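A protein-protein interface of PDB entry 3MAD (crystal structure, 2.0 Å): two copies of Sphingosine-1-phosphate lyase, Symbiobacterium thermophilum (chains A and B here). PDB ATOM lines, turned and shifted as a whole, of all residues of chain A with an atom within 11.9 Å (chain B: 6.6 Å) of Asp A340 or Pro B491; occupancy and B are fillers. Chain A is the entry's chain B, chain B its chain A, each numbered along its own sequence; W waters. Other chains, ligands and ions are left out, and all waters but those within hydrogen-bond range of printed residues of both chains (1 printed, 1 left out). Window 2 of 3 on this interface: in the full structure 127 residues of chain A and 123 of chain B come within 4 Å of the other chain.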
ATOM      1  N   TYR A 335     -28.967 -17.688 -20.493  1.00  0.00           N
ATOM      2  CA  TYR A 335     -29.171 -17.791 -19.057  1.00  0.00           C
ATOM      3  C   TYR A 335     -27.879 -18.134 -18.324  1.00  0.00           C
ATOM      4  O   TYR A 335     -27.000 -18.789 -18.874  1.00  0.00           O
ATOM      5  CB  TYR A 335     -30.235 -18.833 -18.728  1.00  0.00           C
ATOM      6  CG  TYR A 335     -31.599 -18.558 -19.320  1.00  0.00           C
ATOM      7  CD1 TYR A 335     -31.968 -17.278 -19.715  1.00  0.00           C
ATOM      8  CD2 TYR A 335     -32.529 -19.581 -19.460  1.00  0.00           C
ATOM      9  CE1 TYR A 335     -33.223 -17.034 -20.248  1.00  0.00           C
ATOM     10  CE2 TYR A 335     -33.777 -19.349 -19.992  1.00  0.00           C
ATOM     11  CZ  TYR A 335     -34.122 -18.075 -20.381  1.00  0.00           C
ATOM     12  OH  TYR A 335     -35.368 -17.851 -20.907  1.00  0.00           O
ATOM     13  N   PHE A 336     -27.757 -17.666 -17.086  1.00  0.00           N
ATOM     14  CA  PHE A 336     -26.690 -18.126 -16.207  1.00  0.00           C
ATOM     15  C   PHE A 336     -27.329 -18.887 -15.071  1.00  0.00           C
ATOM     16  O   PHE A 336     -28.247 -18.387 -14.428  1.00  0.00           O
ATOM     17  CB  PHE A 336     -25.877 -16.979 -15.617  1.00  0.00           C
ATOM     18  CG  PHE A 336     -24.978 -17.413 -14.489  1.00  0.00           C
ATOM     19  CD1 PHE A 336     -23.809 -18.115 -14.752  1.00  0.00           C
ATOM     20  CD2 PHE A 336     -25.314 -17.144 -13.166  1.00  0.00           C
ATOM     21  CE1 PHE A 336     -22.979 -18.535 -13.713  1.00  0.00           C
ATOM     22  CE2 PHE A 336     -24.494 -17.553 -12.125  1.00  0.00           C
ATOM     23  CZ  PHE A 336     -23.321 -18.254 -12.401  1.00  0.00           C
ATOM     24  N   ILE A 337     -26.857 -20.103 -14.831  1.00  0.00           N
ATOM     25  CA  ILE A 337     -27.383 -20.902 -13.733  1.00  0.00           C
ATOM     26  C   ILE A 337     -26.254 -21.509 -12.910  1.00  0.00           C
ATOM     27  O   ILE A 337     -25.368 -22.181 -13.446  1.00  0.00           O
ATOM     28  CB  ILE A 337     -28.333 -22.006 -14.240  1.00  0.00           C
ATOM     29  CG1 ILE A 337     -29.524 -21.371 -14.971  1.00  0.00           C
ATOM     30  CG2 ILE A 337     -28.793 -22.891 -13.081  1.00  0.00           C
ATOM     31  CD1 ILE A 337     -30.363 -22.343 -15.779  1.00  0.00           C
ATOM     32  N   ALA A 338     -26.288 -21.251 -11.607  1.00  0.00           N
ATOM     33  CA  ALA A 338     -25.318 -21.812 -10.677  1.00  0.00           C
ATOM     34  C   ALA A 338     -26.014 -22.835  -9.792  1.00  0.00           C
ATOM     35  O   ALA A 338     -26.919 -22.491  -9.023  1.00  0.00           O
ATOM     36  CB  ALA A 338     -24.695 -20.709  -9.830  1.00  0.00           C
ATOM     37  N   ALA A 339     -25.599 -24.093  -9.895  1.00  0.00           N
ATOM     38  CA  ALA A 339     -26.277 -25.167  -9.173  1.00  0.00           C
ATOM     39  C   ALA A 339     -25.567 -25.671  -7.909  1.00  0.00           C
ATOM     40  O   ALA A 339     -26.196 -26.288  -7.056  1.00  0.00           O
ATOM     41  CB  ALA A 339     -26.571 -26.338 -10.119  1.00  0.00           C
ATOM     42  N   ASP A 340     -24.271 -25.381  -7.804  1.00  0.00           N
ATOM     43  CA  ASP A 340     -23.411 -25.942  -6.759  1.00  0.00           C
ATOM     44  C   ASP A 340     -22.969 -24.921  -5.705  1.00  0.00           C
ATOM     45  O   ASP A 340     -22.151 -25.236  -4.842  1.00  0.00           O
ATOM     46  CB  ASP A 340     -22.150 -26.549  -7.392  1.00  0.00           C
ATOM     47  CG  ASP A 340     -22.413 -27.871  -8.088  1.00  0.00           C
ATOM     48  OD1 ASP A 340     -22.098 -27.979  -9.292  1.00  0.00           O
ATOM     49  OD2 ASP A 340     -22.927 -28.801  -7.433  1.00  0.00           O
ATOM     50  N   TRP A 341     -23.492 -23.701  -5.781  1.00  0.00           N
ATOM     51  CA  TRP A 341     -23.035 -22.627  -4.910  1.00  0.00           C
ATOM     52  C   TRP A 341     -23.717 -22.751  -3.558  1.00  0.00           C
ATOM     53  O   TRP A 341     -24.935 -22.875  -3.498  1.00  0.00           O
ATOM     54  CB  TRP A 341     -23.334 -21.278  -5.544  1.00  0.00           C
ATOM     55  CG  TRP A 341     -22.857 -20.083  -4.768  1.00  0.00           C
ATOM     56  CD1 TRP A 341     -21.598 -19.867  -4.271  1.00  0.00           C
ATOM     57  CD2 TRP A 341     -23.622 -18.924  -4.439  1.00  0.00           C
ATOM     58  NE1 TRP A 341     -21.542 -18.645  -3.640  1.00  0.00           N
ATOM     59  CE2 TRP A 341     -22.775 -18.048  -3.730  1.00  0.00           C
ATOM     60  CE3 TRP A 341     -24.952 -18.543  -4.665  1.00  0.00           C
ATOM     61  CZ2 TRP A 341     -23.213 -16.815  -3.250  1.00  0.00           C
ATOM     62  CZ3 TRP A 341     -25.380 -17.320  -4.192  1.00  0.00           C
ATOM     63  CH2 TRP A 341     -24.514 -16.468  -3.492  1.00  0.00           C
ATOM     64  N   PRO A 342     -22.925 -22.740  -2.473  1.00  0.00           N
ATOM     65  CA  PRO A 342     -23.443 -22.844  -1.104  1.00  0.00           C
ATOM     66  C   PRO A 342     -24.488 -21.774  -0.790  1.00  0.00           C
ATOM     67  O   PRO A 342     -25.248 -21.929   0.163  1.00  0.00           O
ATOM     68  CB  PRO A 342     -22.194 -22.632  -0.242  1.00  0.00           C
ATOM     69  CG  PRO A 342     -21.069 -23.073  -1.094  1.00  0.00           C
ATOM     70  CD  PRO A 342     -21.453 -22.736  -2.511  1.00  0.00           C
ATOM     71  N   GLY A 343     -24.522 -20.708  -1.587  1.00  0.00           N
ATOM     72  CA  GLY A 343     -25.497 -19.653  -1.410  1.00  0.00           C
ATOM     73  C   GLY A 343     -26.859 -20.043  -1.953  1.00  0.00           C
ATOM     74  O   GLY A 343     -27.775 -19.226  -1.976  1.00  0.00           O
ATOM     75  N   GLY A 344     -26.998 -21.292  -2.391  1.00  0.00           N
ATOM     76  CA  GLY A 344     -28.276 -21.782  -2.878  1.00  0.00           C
ATOM     77  C   GLY A 344     -28.396 -21.679  -4.384  1.00  0.00           C
ATOM     78  O   GLY A 344     -27.465 -21.244  -5.062  1.00  0.00           O
ATOM     79  N   LEU A 345     -29.538 -22.091  -4.921  1.00  0.00           N
ATOM     80  CA  LEU A 345     -29.774 -21.971  -6.348  1.00  0.00           C
ATOM     81  C   LEU A 345     -29.674 -20.508  -6.746  1.00  0.00           C
ATOM     82  O   LEU A 345     -30.175 -19.628  -6.043  1.00  0.00           O
ATOM     83  CB  LEU A 345     -31.151 -22.515  -6.721  1.00  0.00           C
ATOM     84  CG  LEU A 345     -31.358 -24.021  -6.554  1.00  0.00           C
ATOM     85  CD1 LEU A 345     -32.642 -24.437  -7.241  1.00  0.00           C
ATOM     86  CD2 LEU A 345     -30.176 -24.802  -7.114  1.00  0.00           C
ATOM     87  N   TYR A 346     -29.019 -20.254  -7.871  1.00  0.00           N
ATOM     88  CA  TYR A 346     -28.853 -18.899  -8.374  1.00  0.00           C
ATOM     89  C   TYR A 346     -28.946 -18.907  -9.893  1.00  0.00           C
ATOM     90  O   TYR A 346     -28.371 -19.762 -10.563  1.00  0.00           O
ATOM     91  CB  TYR A 346     -27.507 -18.322  -7.926  1.00  0.00           C
ATOM     92  CG  TYR A 346     -27.315 -16.853  -8.238  1.00  0.00           C
ATOM     93  CD1 TYR A 346     -27.682 -15.877  -7.323  1.00  0.00           C
ATOM     94  CD2 TYR A 346     -26.759 -16.445  -9.446  1.00  0.00           C
ATOM     95  CE1 TYR A 346     -27.510 -14.534  -7.600  1.00  0.00           C
ATOM     96  CE2 TYR A 346     -26.583 -15.105  -9.734  1.00  0.00           C
ATOM     97  CZ  TYR A 346     -26.962 -14.153  -8.803  1.00  0.00           C
ATOM     98  OH  TYR A 346     -26.790 -12.811  -9.075  1.00  0.00           O
ATOM     99  N   PHE A 347     -29.691 -17.958 -10.435  1.00  0.00           N
ATOM    100  CA  PHE A 347     -29.798 -17.807 -11.872  1.00  0.00           C
ATOM    101  C   PHE A 347     -30.101 -16.358 -12.188  1.00  0.00           C
ATOM    102  O   PHE A 347     -30.698 -15.648 -11.384  1.00  0.00           O
ATOM    103  CB  PHE A 347     -30.904 -18.704 -12.425  1.00  0.00           C
ATOM    104  CG  PHE A 347     -32.265 -18.410 -11.855  1.00  0.00           C
ATOM    105  CD1 PHE A 347     -32.692 -19.033 -10.692  1.00  0.00           C
ATOM    106  CD2 PHE A 347     -33.115 -17.514 -12.481  1.00  0.00           C
ATOM    107  CE1 PHE A 347     -33.944 -18.768 -10.159  1.00  0.00           C
ATOM    108  CE2 PHE A 347     -34.372 -17.240 -11.953  1.00  0.00           C
ATOM    109  CZ  PHE A 347     -34.787 -17.871 -10.790  1.00  0.00           C
ATOM    110  N   VAL B 199     -14.971 -21.591  -2.112  1.00  0.00           N
ATOM    111  CA  VAL B 199     -16.235 -22.125  -2.623  1.00  0.00           C
ATOM    112  C   VAL B 199     -17.426 -21.240  -2.248  1.00  0.00           C
ATOM    113  O   VAL B 199     -18.445 -21.239  -2.946  1.00  0.00           O
ATOM    114  CB  VAL B 199     -16.505 -23.570  -2.132  1.00  0.00           C
ATOM    115  CG1 VAL B 199     -15.500 -24.525  -2.738  1.00  0.00           C
ATOM    116  CG2 VAL B 199     -16.460 -23.633  -0.607  1.00  0.00           C
ATOM    117  N   HIS B 436     -27.731 -24.478   0.488  1.00  0.00           N
ATOM    118  CA  HIS B 436     -27.342 -25.883   0.571  1.00  0.00           C
ATOM    119  C   HIS B 436     -25.827 -25.957   0.593  1.00  0.00           C
ATOM    120  O   HIS B 436     -25.158 -24.942   0.410  1.00  0.00           O
ATOM    121  CB  HIS B 436     -27.922 -26.719  -0.572  1.00  0.00           C
ATOM    122  CG  HIS B 436     -27.611 -26.189  -1.938  1.00  0.00           C
ATOM    123  ND1 HIS B 436     -28.541 -26.175  -2.957  1.00  0.00           N
ATOM    124  CD2 HIS B 436     -26.480 -25.653  -2.453  1.00  0.00           C
ATOM    125  CE1 HIS B 436     -27.991 -25.659  -4.044  1.00  0.00           C
ATOM    126  NE2 HIS B 436     -26.742 -25.331  -3.762  1.00  0.00           N
ATOM    127  N   ARG B 437     -25.292 -27.149   0.837  1.00  0.00           N
ATOM    128  CA  ARG B 437     -23.851 -27.336   1.015  1.00  0.00           C
ATOM    129  C   ARG B 437     -23.278 -26.489   2.149  1.00  0.00           C
ATOM    130  O   ARG B 437     -22.342 -25.728   1.926  1.00  0.00           O
ATOM    131  CB  ARG B 437     -23.097 -27.011  -0.278  1.00  0.00           C
ATOM    132  CG  ARG B 437     -23.269 -28.040  -1.375  1.00  0.00           C
ATOM    133  CD  ARG B 437     -22.750 -27.497  -2.688  1.00  0.00           C
ATOM    134  NE  ARG B 437     -21.339 -27.116  -2.617  1.00  0.00           N
ATOM    135  CZ  ARG B 437     -20.356 -27.767  -3.233  1.00  0.00           C
ATOM    136  NH1 ARG B 437     -20.628 -28.841  -3.968  1.00  0.00           N
ATOM    137  NH2 ARG B 437     -19.103 -27.345  -3.118  1.00  0.00           N
ATOM    138  N   ALA B 489     -30.073 -33.190  -6.384  1.00  0.00           N
ATOM    139  CA  ALA B 489     -30.095 -33.356  -7.837  1.00  0.00           C
ATOM    140  C   ALA B 489     -28.741 -33.080  -8.483  1.00  0.00           C
ATOM    141  O   ALA B 489     -27.946 -32.304  -7.960  1.00  0.00           O
ATOM    142  CB  ALA B 489     -31.149 -32.449  -8.444  1.00  0.00           C
ATOM    143  N   PRO B 490     -28.477 -33.720  -9.632  1.00  0.00           N
ATOM    144  CA  PRO B 490     -27.294 -33.422 -10.443  1.00  0.00           C
ATOM    145  C   PRO B 490     -27.397 -32.028 -11.052  1.00  0.00           C
ATOM    146  O   PRO B 490     -28.459 -31.671 -11.556  1.00  0.00           O
ATOM    147  CB  PRO B 490     -27.361 -34.473 -11.557  1.00  0.00           C
ATOM    148  CG  PRO B 490     -28.228 -35.550 -11.024  1.00  0.00           C
ATOM    149  CD  PRO B 490     -29.245 -34.846 -10.184  1.00  0.00           C
ATOM    150  N   PRO B 491     -26.297 -31.257 -11.021  1.00  0.00           N
ATOM    151  CA  PRO B 491     -26.288 -29.882 -11.528  1.00  0.00           C
ATOM    152  C   PRO B 491     -26.898 -29.756 -12.924  1.00  0.00           C
ATOM    153  O   PRO B 491     -27.644 -28.809 -13.172  1.00  0.00           O
ATOM    154  CB  PRO B 491     -24.797 -29.538 -11.561  1.00  0.00           C
ATOM    155  CG  PRO B 491     -24.215 -30.355 -10.464  1.00  0.00           C
ATOM    156  CD  PRO B 491     -24.978 -31.655 -10.498  1.00  0.00           C
ATOM    157  N   GLU B 492     -26.596 -30.691 -13.817  1.00  0.00           N
ATOM    158  CA  GLU B 492     -27.119 -30.607 -15.174  1.00  0.00           C
ATOM    159  C   GLU B 492     -28.642 -30.653 -15.145  1.00  0.00           C
ATOM    160  O   GLU B 492     -29.309 -29.950 -15.906  1.00  0.00           O
ATOM    161  CB  GLU B 492     -26.571 -31.737 -16.048  1.00  0.00           C
ATOM    162  CG  GLU B 492     -25.939 -31.267 -17.365  1.00  0.00           C
ATOM    163  CD  GLU B 492     -26.720 -30.154 -18.058  1.00  0.00           C
ATOM    164  OE1 GLU B 492     -27.953 -30.286 -18.227  1.00  0.00           O
ATOM    165  OE2 GLU B 492     -26.091 -29.146 -18.450  1.00  0.00           O
ATOM    166  N   LEU B 493     -29.186 -31.477 -14.254  1.00  0.00           N
ATOM    167  CA  LEU B 493     -30.635 -31.615 -14.114  1.00  0.00           C
ATOM    168  C   LEU B 493     -31.251 -30.324 -13.576  1.00  0.00           C
ATOM    169  O   LEU B 493     -32.273 -29.844 -14.074  1.00  0.00           O
ATOM    170  CB  LEU B 493     -30.973 -32.795 -13.195  1.00  0.00           C
ATOM    171  CG  LEU B 493     -32.432 -33.255 -13.105  1.00  0.00           C
ATOM    172  CD1 LEU B 493     -33.232 -32.363 -12.180  1.00  0.00           C
ATOM    173  CD2 LEU B 493     -33.075 -33.312 -14.487  1.00  0.00           C
ATOM    174  N   VAL B 494     -30.626 -29.771 -12.544  1.00  0.00           N
ATOM    175  CA  VAL B 494     -31.044 -28.488 -12.006  1.00  0.00           C
ATOM    176  C   VAL B 494     -31.006 -27.435 -13.112  1.00  0.00           C
ATOM    177  O   VAL B 494     -31.946 -26.667 -13.290  1.00  0.00           O
ATOM    178  CB  VAL B 494     -30.133 -28.062 -10.847  1.00  0.00           C
ATOM    179  CG1 VAL B 494     -30.528 -26.683 -10.332  1.00  0.00           C
ATOM    180  CG2 VAL B 494     -30.196 -29.094  -9.739  1.00  0.00           C
ATOM    181  N   ARG B 495     -29.915 -27.421 -13.864  1.00  0.00           N
ATOM    182  CA  ARG B 495     -29.745 -26.473 -14.957  1.00  0.00           C
ATOM    183  C   ARG B 495     -30.934 -26.509 -15.912  1.00  0.00           C
ATOM    184  O   ARG B 495     -31.467 -25.466 -16.288  1.00  0.00           O
ATOM    185  CB  ARG B 495     -28.440 -26.753 -15.702  1.00  0.00           C
ATOM    186  CG  ARG B 495     -28.060 -25.702 -16.733  1.00  0.00           C
ATOM    187  CD  ARG B 495     -26.546 -25.679 -16.960  1.00  0.00           C
ATOM    188  NE  ARG B 495     -25.808 -25.456 -15.715  1.00  0.00           N
ATOM    189  CZ  ARG B 495     -24.983 -26.341 -15.158  1.00  0.00           C
ATOM    190  NH1 ARG B 495     -24.771 -27.515 -15.742  1.00  0.00           N
ATOM    191  NH2 ARG B 495     -24.361 -26.049 -14.021  1.00  0.00           N
ATOM    192  N   GLN B 496     -31.358 -27.711 -16.285  1.00  0.00           N
ATOM    193  CA  GLN B 496     -32.477 -27.871 -17.211  1.00  0.00           C
ATOM    194  C   GLN B 496     -33.801 -27.436 -16.592  1.00  0.00           C
ATOM    195  O   GLN B 496     -34.588 -26.730 -17.226  1.00  0.00           O
ATOM    196  CB  GLN B 496     -32.557 -29.316 -17.708  1.00  0.00           C
ATOM    197  CG  GLN B 496     -31.345 -29.723 -18.541  1.00  0.00           C
ATOM    198  CD  GLN B 496     -31.327 -31.202 -18.887  1.00  0.00           C
ATOM    199  OE1 GLN B 496     -32.238 -31.952 -18.528  1.00  0.00           O
ATOM    200  NE2 GLN B 496     -30.281 -31.630 -19.591  1.00  0.00           N
HETATM  201  O   HOH W   1     -24.879 -23.277   2.980  1.00  0.00           O
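A ring nitrogen (NE2) of His B436 sits at hydrogen-bond distance from the backbone carbonyl oxygen (O) of Ala A339 (3.5 Å). A ring nitrogen (NE2) of His B436 lies within hydrogen-bond range of the backbone carbonyl oxygen (O) of Trp A341, at 3.1 Å. The backbone carbonyl oxygen (O) of Asp A340 is in hydrogen-bond range of the guanidinium group (NE) of Arg B437 (3.0 Å). The backbone carbonyl oxygen (O) of Pro A342 lies close to the backbone carbonyl oxygen (O) of His B436, at 3.0 Å.
NH1 of Arg B495 is in salt-bridge range of OE2 of Glu B492 (3.4 Å).
Among the printed residues, pairs that only touch across the chains: Ile A337 with Arg B495 (3.4 Å), Pro A342 with Val B199 (3.4 Å), Asp A340 with Pro B491 (3.4 Å), Trp A341 with Val B199 (3.7 Å), Leu A345 with Val B494 (3.7 Å), Pro A342 with Arg B437 (3.8 Å), Ala A339 with Pro B491 (3.8 Å), Leu A345 with His B436 (3.9 Å), Gly A344 with His B436 (3.97 Å) and Ala A339 with Val B494 (3.98 Å).
Printed residues of chain B within 4 Å of Ala A339: His B436 (3.5 Å), Pro B491 (3.8 Å) and Val B494 (3.98 Å). Printed residues of chain B within 4 Å of Asp A340: Arg B437 and Pro B491. Of the printed residues of chain B, Gly A344 touches His B436. Of the printed residues of chain A, Val B199 touches Trp A341 and Pro A342. His B436 touches just these residues of chain A: Ala A339 (3.5 Å), Trp A341 (3.1 Å), Pro A342 (3.0 Å), Gly A344 (3.97 Å) and Leu A345 (3.9 Å). No residue of chain A comes within 4 Å of Ala B489. No residue of chain A comes within 4 Å of Pro B490. Of the printed residues of chain A, Pro B491 touches Ala A339 and Asp A340. No residue of chain A comes within 4 Å of Leu B493. Val B494 touches just these residues of chain A: Ala A339 and Leu A345. The nearest printed residue of chain B that does not touch Asp A340 is His B436 (4.3 Å). The nearest printed residue of chain A that does not touch Pro B491 is Ile A337 (6.0 Å). The nearest printed residue of chain B that does not touch Trp A341 is Arg B437 (4.9 Å).
Of the 11 printed residues of chain B, 6 touch a printed residue of chain A. Hydrophobic or aromatic side chains of chain A that line the printed part of chain B: Ile A337, Ala A339, Trp A341, Pro A342 and Leu A345. Among the printed residues, 14 pairs touch across the chains. Among the printed residues, no Asp or Glu carboxylate lies within 4 Å of a Lys or Arg side-chain nitrogen of the other chain.
No position is printed for both chains. Of the 14 pairs that touch across the chains among the printed residues, none has its exchanged pair printed and touching as well.
Water W1 bridges O of His B436 (3.1 Å) and O of Pro A342 (3.1 Å).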
